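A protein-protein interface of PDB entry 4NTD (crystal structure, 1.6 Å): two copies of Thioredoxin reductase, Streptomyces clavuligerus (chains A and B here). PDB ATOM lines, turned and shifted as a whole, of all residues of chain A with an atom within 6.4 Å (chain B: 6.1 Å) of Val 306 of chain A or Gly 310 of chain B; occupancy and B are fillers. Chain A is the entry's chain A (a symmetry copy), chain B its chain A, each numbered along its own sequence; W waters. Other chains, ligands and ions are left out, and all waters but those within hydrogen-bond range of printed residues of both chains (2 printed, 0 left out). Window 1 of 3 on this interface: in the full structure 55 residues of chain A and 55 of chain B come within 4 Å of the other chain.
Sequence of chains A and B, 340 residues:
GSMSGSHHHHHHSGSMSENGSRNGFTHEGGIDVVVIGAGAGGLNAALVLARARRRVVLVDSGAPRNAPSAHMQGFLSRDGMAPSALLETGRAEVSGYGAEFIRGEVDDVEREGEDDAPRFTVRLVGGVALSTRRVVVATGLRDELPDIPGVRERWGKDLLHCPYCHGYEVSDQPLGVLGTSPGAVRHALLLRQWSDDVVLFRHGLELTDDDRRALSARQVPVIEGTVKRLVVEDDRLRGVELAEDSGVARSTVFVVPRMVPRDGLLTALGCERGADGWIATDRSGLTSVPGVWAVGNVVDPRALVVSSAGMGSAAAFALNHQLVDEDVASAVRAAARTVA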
ATOM      1  N   ALA A  40     -20.982  22.535  -0.245  1.00  0.00           N
ATOM      2  CA  ALA A  40     -20.691  21.595   0.840  1.00  0.00           C
ATOM      3  C   ALA A  40     -19.833  20.411   0.375  1.00  0.00           C
ATOM      4  O   ALA A  40     -18.997  19.914   1.132  1.00  0.00           O
ATOM      5  CB  ALA A  40     -21.978  21.101   1.479  1.00  0.00           C
ATOM      6  N   MET A  72     -31.464  26.705   5.042  1.00  0.00           N
ATOM      7  CA  MET A  72     -31.431  25.298   4.658  1.00  0.00           C
ATOM      8  C   MET A  72     -31.940  24.436   5.809  1.00  0.00           C
ATOM      9  O   MET A  72     -31.811  24.798   6.981  1.00  0.00           O
ATOM     10  CB  MET A  72     -30.041  24.849   4.186  1.00  0.00           C
ATOM     11  CG  MET A  72     -28.970  24.738   5.253  1.00  0.00           C
ATOM     12  SD  MET A  72     -27.807  23.377   4.979  1.00  0.00           S
ATOM     13  CE  MET A  72     -26.870  23.538   6.495  1.00  0.00           C
ATOM     14  N   GLY A  74     -32.561  20.179   7.261  1.00  0.00           N
ATOM     15  CA  GLY A  74     -32.276  18.744   7.177  1.00  0.00           C
ATOM     16  C   GLY A  74     -30.821  18.307   7.296  1.00  0.00           C
ATOM     17  O   GLY A  74     -30.519  17.131   7.117  1.00  0.00           O
ATOM     18  N   PHE A  75     -29.930  19.250   7.600  1.00  0.00           N
ATOM     19  CA  PHE A  75     -28.495  18.993   7.794  1.00  0.00           C
ATOM     20  C   PHE A  75     -28.261  18.858   9.301  1.00  0.00           C
ATOM     21  O   PHE A  75     -28.480  19.811  10.046  1.00  0.00           O
ATOM     22  CB  PHE A  75     -27.720  20.189   7.218  1.00  0.00           C
ATOM     23  CG  PHE A  75     -26.213  20.042   7.194  1.00  0.00           C
ATOM     24  CD1 PHE A  75     -25.532  20.037   5.982  1.00  0.00           C
ATOM     25  CD2 PHE A  75     -25.467  19.994   8.368  1.00  0.00           C
ATOM     26  CE1 PHE A  75     -24.149  19.946   5.936  1.00  0.00           C
ATOM     27  CE2 PHE A  75     -24.082  19.901   8.328  1.00  0.00           C
ATOM     28  CZ  PHE A  75     -23.423  19.874   7.113  1.00  0.00           C
ATOM     29  N   LEU A  76     -27.823  17.680   9.746  1.00  0.00           N
ATOM     30  CA  LEU A  76     -27.703  17.394  11.183  1.00  0.00           C
ATOM     31  C   LEU A  76     -26.917  18.468  11.942  1.00  0.00           C
ATOM     32  O   LEU A  76     -25.777  18.777  11.595  1.00  0.00           O
ATOM     33  CB  LEU A  76     -27.048  16.029  11.420  1.00  0.00           C
ATOM     34  CG  LEU A  76     -26.999  15.560  12.878  1.00  0.00           C
ATOM     35  CD1 LEU A  76     -28.400  15.260  13.390  1.00  0.00           C
ATOM     36  CD2 LEU A  76     -26.098  14.344  13.017  1.00  0.00           C
ATOM     37  N   ALA A 303     -28.805  14.392  -4.101  1.00  0.00           N
ATOM     38  CA  ALA A 303     -27.903  14.708  -2.989  1.00  0.00           C
ATOM     39  C   ALA A 303     -28.255  16.033  -2.314  1.00  0.00           C
ATOM     40  O   ALA A 303     -27.991  17.108  -2.855  1.00  0.00           O
ATOM     41  CB  ALA A 303     -26.454  14.722  -3.461  1.00  0.00           C
ATOM     42  N   LEU A 304     -28.858  15.940  -1.133  1.00  0.00           N
ATOM     43  CA  LEU A 304     -29.095  17.106  -0.285  1.00  0.00           C
ATOM     44  C   LEU A 304     -27.750  17.586   0.280  1.00  0.00           C
ATOM     45  O   LEU A 304     -26.718  16.950   0.056  1.00  0.00           O
ATOM     46  CB  LEU A 304     -30.103  16.763   0.819  1.00  0.00           C
ATOM     47  CG  LEU A 304     -31.513  16.441   0.299  1.00  0.00           C
ATOM     48  CD1 LEU A 304     -32.330  15.647   1.307  1.00  0.00           C
ATOM     49  CD2 LEU A 304     -32.248  17.714  -0.099  1.00  0.00           C
ATOM     50  N   VAL A 305     -27.748  18.707   0.995  1.00  0.00           N
ATOM     51  CA  VAL A 305     -26.488  19.362   1.362  1.00  0.00           C
ATOM     52  C   VAL A 305     -25.597  18.445   2.207  1.00  0.00           C
ATOM     53  O   VAL A 305     -24.403  18.306   1.930  1.00  0.00           O
ATOM     54  CB  VAL A 305     -26.718  20.715   2.078  1.00  0.00           C
ATOM     55  CG1 VAL A 305     -25.399  21.326   2.532  1.00  0.00           C
ATOM     56  CG2 VAL A 305     -27.427  21.695   1.151  1.00  0.00           C
ATOM     57  N   VAL A 306     -26.177  17.806   3.219  1.00  0.00           N
ATOM     58  CA  VAL A 306     -25.393  16.938   4.099  1.00  0.00           C
ATOM     59  C   VAL A 306     -24.866  15.701   3.356  1.00  0.00           C
ATOM     60  O   VAL A 306     -23.784  15.198   3.675  1.00  0.00           O
ATOM     61  CB  VAL A 306     -26.172  16.549   5.383  1.00  0.00           C
ATOM     62  CG1 VAL A 306     -27.283  15.548   5.088  1.00  0.00           C
ATOM     63  CG2 VAL A 306     -25.220  16.016   6.447  1.00  0.00           C
ATOM     64  N   SER A 307     -25.612  15.219   2.364  1.00  0.00           N
ATOM     65  CA  SER A 307     -25.143  14.101   1.533  1.00  0.00           C
ATOM     66  C   SER A 307     -23.979  14.520   0.634  1.00  0.00           C
ATOM     67  O   SER A 307     -23.053  13.739   0.396  1.00  0.00           O
ATOM     68  CB  SER A 307     -26.281  13.513   0.698  1.00  0.00           C
ATOM     69  OG  SER A 307     -27.254  12.896   1.524  1.00  0.00           O
ATOM     70  N   SER A 308     -24.021  15.754   0.140  1.00  0.00           N
ATOM     71  CA  SER A 308     -22.920  16.292  -0.650  1.00  0.00           C
ATOM     72  C   SER A 308     -21.658  16.434   0.208  1.00  0.00           C
ATOM     73  O   SER A 308     -20.572  16.046  -0.216  1.00  0.00           O
ATOM     74  CB  SER A 308     -23.320  17.624  -1.286  1.00  0.00           C
ATOM     75  OG  SER A 308     -24.424  17.433  -2.158  1.00  0.00           O
ATOM     76  N   ALA A 309     -21.810  16.960   1.423  1.00  0.00           N
ATOM     77  CA  ALA A 309     -20.698  17.026   2.375  1.00  0.00           C
ATOM     78  C   ALA A 309     -20.146  15.631   2.662  1.00  0.00           C
ATOM     79  O   ALA A 309     -18.929  15.425   2.667  1.00  0.00           O
ATOM     80  CB  ALA A 309     -21.140  17.693   3.670  1.00  0.00           C
ATOM     81  N   GLY A 310     -21.048  14.679   2.891  1.00  0.00           N
ATOM     82  CA  GLY A 310     -20.668  13.292   3.155  1.00  0.00           C
ATOM     83  C   GLY A 310     -19.857  12.673   2.031  1.00  0.00           C
ATOM     84  O   GLY A 310     -18.877  11.969   2.281  1.00  0.00           O
ATOM     85  N   MET A 311     -20.297  12.930   0.793  1.00  0.00           N
ATOM     86  CA  MET A 311     -19.595  12.502  -0.425  1.00  0.00           C
ATOM     87  C   MET A 311     -18.199  13.117  -0.514  1.00  0.00           C
ATOM     88  O   MET A 311     -17.239  12.446  -0.893  1.00  0.00           O
ATOM     89  CB  MET A 311     -20.391  12.904  -1.678  1.00  0.00           C
ATOM     90  CG  MET A 311     -21.487  11.932  -2.106  1.00  0.00           C
ATOM     91  SD  MET A 311     -22.209  12.358  -3.709  1.00  0.00           S
ATOM     92  CE  MET A 311     -23.689  11.343  -3.708  1.00  0.00           C
ATOM     93  N   ALA B  40     -24.856   9.801  14.175  1.00  0.00           N
ATOM     94  CA  ALA B  40     -25.147  10.747  13.095  1.00  0.00           C
ATOM     95  C   ALA B  40     -25.962  10.110  11.963  1.00  0.00           C
ATOM     96  O   ALA B  40     -26.803  10.773  11.353  1.00  0.00           O
ATOM     97  CB  ALA B  40     -23.862  11.349  12.552  1.00  0.00           C
ATOM     98  N   ASN B  44     -29.671  11.715  11.305  1.00  0.00           N
ATOM     99  CA  ASN B  44     -29.969  12.453  10.075  1.00  0.00           C
ATOM    100  C   ASN B  44     -31.071  11.761   9.261  1.00  0.00           C
ATOM    101  O   ASN B  44     -31.850  12.433   8.583  1.00  0.00           O
ATOM    102  CB  ASN B  44     -28.714  12.724   9.234  1.00  0.00           C
ATOM    103  CG  ASN B  44     -28.756  14.082   8.536  1.00  0.00           C
ATOM    104  OD1 ASN B  44     -27.775  14.827   8.540  1.00  0.00           O
ATOM    105  ND2 ASN B  44     -29.899  14.413   7.942  1.00  0.00           N
ATOM    106  N   PHE B  75     -16.006  17.381  10.096  1.00  0.00           N
ATOM    107  CA  PHE B  75     -17.438  17.503   9.784  1.00  0.00           C
ATOM    108  C   PHE B  75     -17.703  18.972   9.447  1.00  0.00           C
ATOM    109  O   PHE B  75     -17.525  19.841  10.300  1.00  0.00           O
ATOM    110  CB  PHE B  75     -18.230  17.067  11.027  1.00  0.00           C
ATOM    111  CG  PHE B  75     -19.732  16.986  10.850  1.00  0.00           C
ATOM    112  CD1 PHE B  75     -20.385  15.765  10.988  1.00  0.00           C
ATOM    113  CD2 PHE B  75     -20.504  18.123  10.631  1.00  0.00           C
ATOM    114  CE1 PHE B  75     -21.764  15.672  10.873  1.00  0.00           C
ATOM    115  CE2 PHE B  75     -21.884  18.035  10.513  1.00  0.00           C
ATOM    116  CZ  PHE B  75     -22.514  16.810  10.630  1.00  0.00           C
ATOM    117  N   VAL B 305     -18.022  10.707  10.373  1.00  0.00           N
ATOM    118  CA  VAL B 305     -19.307  11.123  10.946  1.00  0.00           C
ATOM    119  C   VAL B 305     -20.193  11.818   9.906  1.00  0.00           C
ATOM    120  O   VAL B 305     -21.376  11.494   9.778  1.00  0.00           O
ATOM    121  CB  VAL B 305     -19.128  12.016  12.199  1.00  0.00           C
ATOM    122  CG1 VAL B 305     -20.473  12.511  12.715  1.00  0.00           C
ATOM    123  CG2 VAL B 305     -18.424  11.242  13.306  1.00  0.00           C
ATOM    124  N   VAL B 306     -19.620  12.753   9.153  1.00  0.00           N
ATOM    125  CA  VAL B 306     -20.401  13.492   8.160  1.00  0.00           C
ATOM    126  C   VAL B 306     -20.879  12.581   7.019  1.00  0.00           C
ATOM    127  O   VAL B 306     -21.953  12.803   6.454  1.00  0.00           O
ATOM    128  CB  VAL B 306     -19.641  14.734   7.624  1.00  0.00           C
ATOM    129  CG1 VAL B 306     -18.499  14.340   6.696  1.00  0.00           C
ATOM    130  CG2 VAL B 306     -20.603  15.694   6.935  1.00  0.00           C
ATOM    131  N   SER B 307     -20.098  11.554   6.689  1.00  0.00           N
ATOM    132  CA  SER B 307     -20.519  10.572   5.678  1.00  0.00           C
ATOM    133  C   SER B 307     -21.673   9.705   6.185  1.00  0.00           C
ATOM    134  O   SER B 307     -22.572   9.343   5.420  1.00  0.00           O
ATOM    135  CB  SER B 307     -19.347   9.697   5.231  1.00  0.00           C
ATOM    136  OG  SER B 307     -18.378  10.461   4.533  1.00  0.00           O
ATOM    137  N   SER B 308     -21.651   9.377   7.474  1.00  0.00           N
ATOM    138  CA  SER B 308     -22.748   8.637   8.085  1.00  0.00           C
ATOM    139  C   SER B 308     -24.032   9.472   8.085  1.00  0.00           C
ATOM    140  O   SER B 308     -25.098   8.973   7.732  1.00  0.00           O
ATOM    141  CB  SER B 308     -22.368   8.190   9.498  1.00  0.00           C
ATOM    142  OG  SER B 308     -21.239   7.330   9.448  1.00  0.00           O
ATOM    143  N   ALA B 309     -23.922  10.749   8.450  1.00  0.00           N
ATOM    144  CA  ALA B 309     -25.056  11.672   8.366  1.00  0.00           C
ATOM    145  C   ALA B 309     -25.578  11.761   6.933  1.00  0.00           C
ATOM    146  O   ALA B 309     -26.789  11.708   6.701  1.00  0.00           O
ATOM    147  CB  ALA B 309     -24.661  13.055   8.868  1.00  0.00           C
ATOM    148  N   GLY B 310     -24.657  11.888   5.980  1.00  0.00           N
ATOM    149  CA  GLY B 310     -25.006  11.958   4.562  1.00  0.00           C
ATOM    150  C   GLY B 310     -25.775  10.743   4.078  1.00  0.00           C
ATOM    151  O   GLY B 310     -26.744  10.873   3.325  1.00  0.00           O
ATOM    152  N   MET B 311     -25.315   9.560   4.504  1.00  0.00           N
ATOM    153  CA  MET B 311     -25.977   8.279   4.223  1.00  0.00           C
ATOM    154  C   MET B 311     -27.386   8.235   4.813  1.00  0.00           C
ATOM    155  O   MET B 311     -28.320   7.747   4.176  1.00  0.00           O
ATOM    156  CB  MET B 311     -25.164   7.111   4.805  1.00  0.00           C
ATOM    157  CG  MET B 311     -24.034   6.589   3.922  1.00  0.00           C
ATOM    158  SD  MET B 311     -23.286   5.074   4.571  1.00  0.00           S
ATOM    159  CE  MET B 311     -21.780   4.981   3.598  1.00  0.00           C
ATOM    160  N   GLY B 312     -27.522   8.742   6.036  1.00  0.00           N
ATOM    161  CA  GLY B 312     -28.811   8.804   6.728  1.00  0.00           C
ATOM    162  C   GLY B 312     -29.831   9.616   5.946  1.00  0.00           C
ATOM    163  O   GLY B 312     -30.975   9.196   5.776  1.00  0.00           O
ATOM    164  N   SER B 313     -29.404  10.774   5.449  1.00  0.00           N
ATOM    165  CA  SER B 313     -30.261  11.611   4.614  1.00  0.00           C
ATOM    166  C   SER B 313     -30.662  10.888   3.323  1.00  0.00           C
ATOM    167  O   SER B 313     -31.828  10.920   2.928  1.00  0.00           O
ATOM    168  CB  SER B 313     -29.566  12.936   4.284  1.00  0.00           C
ATOM    169  OG  SER B 313     -30.412  13.775   3.517  1.00  0.00           O
ATOM    170  N   ALA B 314     -29.698  10.232   2.677  1.00  0.00           N
ATOM    171  CA  ALA B 314     -29.966   9.502   1.434  1.00  0.00           C
ATOM    172  C   ALA B 314     -30.955   8.354   1.648  1.00  0.00           C
ATOM    173  O   ALA B 314     -31.825   8.112   0.809  1.00  0.00           O
ATOM    174  CB  ALA B 314     -28.672   8.988   0.825  1.00  0.00           C
ATOM    175  N   ALA B 315     -30.824   7.658   2.774  1.00  0.00           N
ATOM    176  CA  ALA B 315     -31.754   6.586   3.126  1.00  0.00           C
ATOM    177  C   ALA B 315     -33.167   7.126   3.338  1.00  0.00           C
ATOM    178  O   ALA B 315     -34.134   6.548   2.842  1.00  0.00           O
ATOM    179  CB  ALA B 315     -31.271   5.849   4.367  1.00  0.00           C
HETATM  180  O   HOH W   1     -30.847  16.383   4.431  1.00  0.00           O
HETATM  181  O   HOH W   2     -29.804  13.232   0.821  1.00  0.00           O
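OD1 of Asn 44 of chain B is in hydrogen-bond range of N of Leu 76 of chain A (3.1 Å). O of Gly 310 of chain B sits at hydrogen-bond distance from OG of Ser 307 of chain A (2.8 Å). The side-chain amide nitrogen (ND2) of Asn 44 of chain B sits at hydrogen-bond distance from the backbone carbonyl oxygen (O) of Gly 74 of chain A (2.9 Å). The side-chain hydroxyl (OG) of Ser 307 of chain B lies within hydrogen-bond range of the backbone carbonyl oxygen (O) of Gly 310 of chain A (2.8 Å).
O of Leu 304 of chain A sits at hydrogen-bond distance from OG of Ser 308 of chain A, at 3.2 Å.
Among the printed residues, pairs that only touch across the chains: Leu 304 of chain A with Ser 313 of chain B, Val 306 of chain A with Asn 44 of chain B, Val 306 of chain A with Ser 313 of chain B, Gly 310 of chain A with Val 306 of chain B, Val 306 of chain A with Gly 310 of chain B, Ser 307 of chain A with Ser 313 of chain B, Phe 75 of chain A with Phe 75 of chain B, Leu 76 of chain A with Ala 40 of chain B, Ser 307 of chain A with Ala 314 of chain B, Val 306 of chain A with Ala 309 of chain B, Ala 309 of chain A with Val 306 of chain B and Leu 76 of chain A with Phe 75 of chain B.
Val 306 of chain A touches four residues of chain B. Of the printed residues of chain A, Gly 310 of chain B touches Val 306 (3.6 Å) and Ser 307 (2.8 Å). Printed residues of chain A within 4 Å of Ser 313 of chain B: Leu 304, Val 306 and Ser 307. Of the printed residues of chain A, Ser 307 of chain B touches Gly 310 (2.8 Å). Of the printed residues of chain B, Leu 304 of chain A touches Ser 313. Of the printed residues of chain A, Val 306 of chain B touches Ala 309 and Gly 310. Printed residues of chain B within 4 Å of Phe 75 of chain A: Phe 75 (3.6 Å). Met 311 of chain B touches none of the printed residues of chain A. The nearest residue of chain B that does not touch Val 306 of chain A is Val 306 of chain B (4.1 Å).
Of the 14 printed residues of chain A, 8 touch a printed residue of chain B. Hydrophobic or aromatic side chains of chain A within 4 Å of the printed part of chain B: Phe 75, Leu 76, Leu 304, Val 306 and Ala 309. Among the printed residues, no Asp or Glu carboxylate lies within 4 Å of a Lys or Arg side-chain nitrogen of the other chain.
Phe 75 of chain B touches its own counterpart, Phe 75 of chain A. Val 306 of chain A touches Ala 309 of chain B, and with the chains exchanged Ala 309 of chain A touches Val 306 of chain B. Val 306 of chain A touches Gly 310 of chain B, and with the chains exchanged Gly 310 of chain A touches Val 306 of chain B. Ser 307 of chain A touches Gly 310 of chain B, and with the chains exchanged Gly 310 of chain A touches Ser 307 of chain B. 9 positions are printed for both chains. Of the 16 pairs that touch across the chains among the printed residues, 7 have their exchanged pair printed and touching as well.
Water W2 lies within hydrogen-bond range of OG of Ser 307 of chain A, OG of Ser 313 of chain B and N of Leu 304 of chain A. Water W1 bridges the side-chain hydroxyl of Ser 313 of chain B (2.8 Å) and the backbone carbonyl oxygen of Gly 74 of chain A (2.8 Å).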
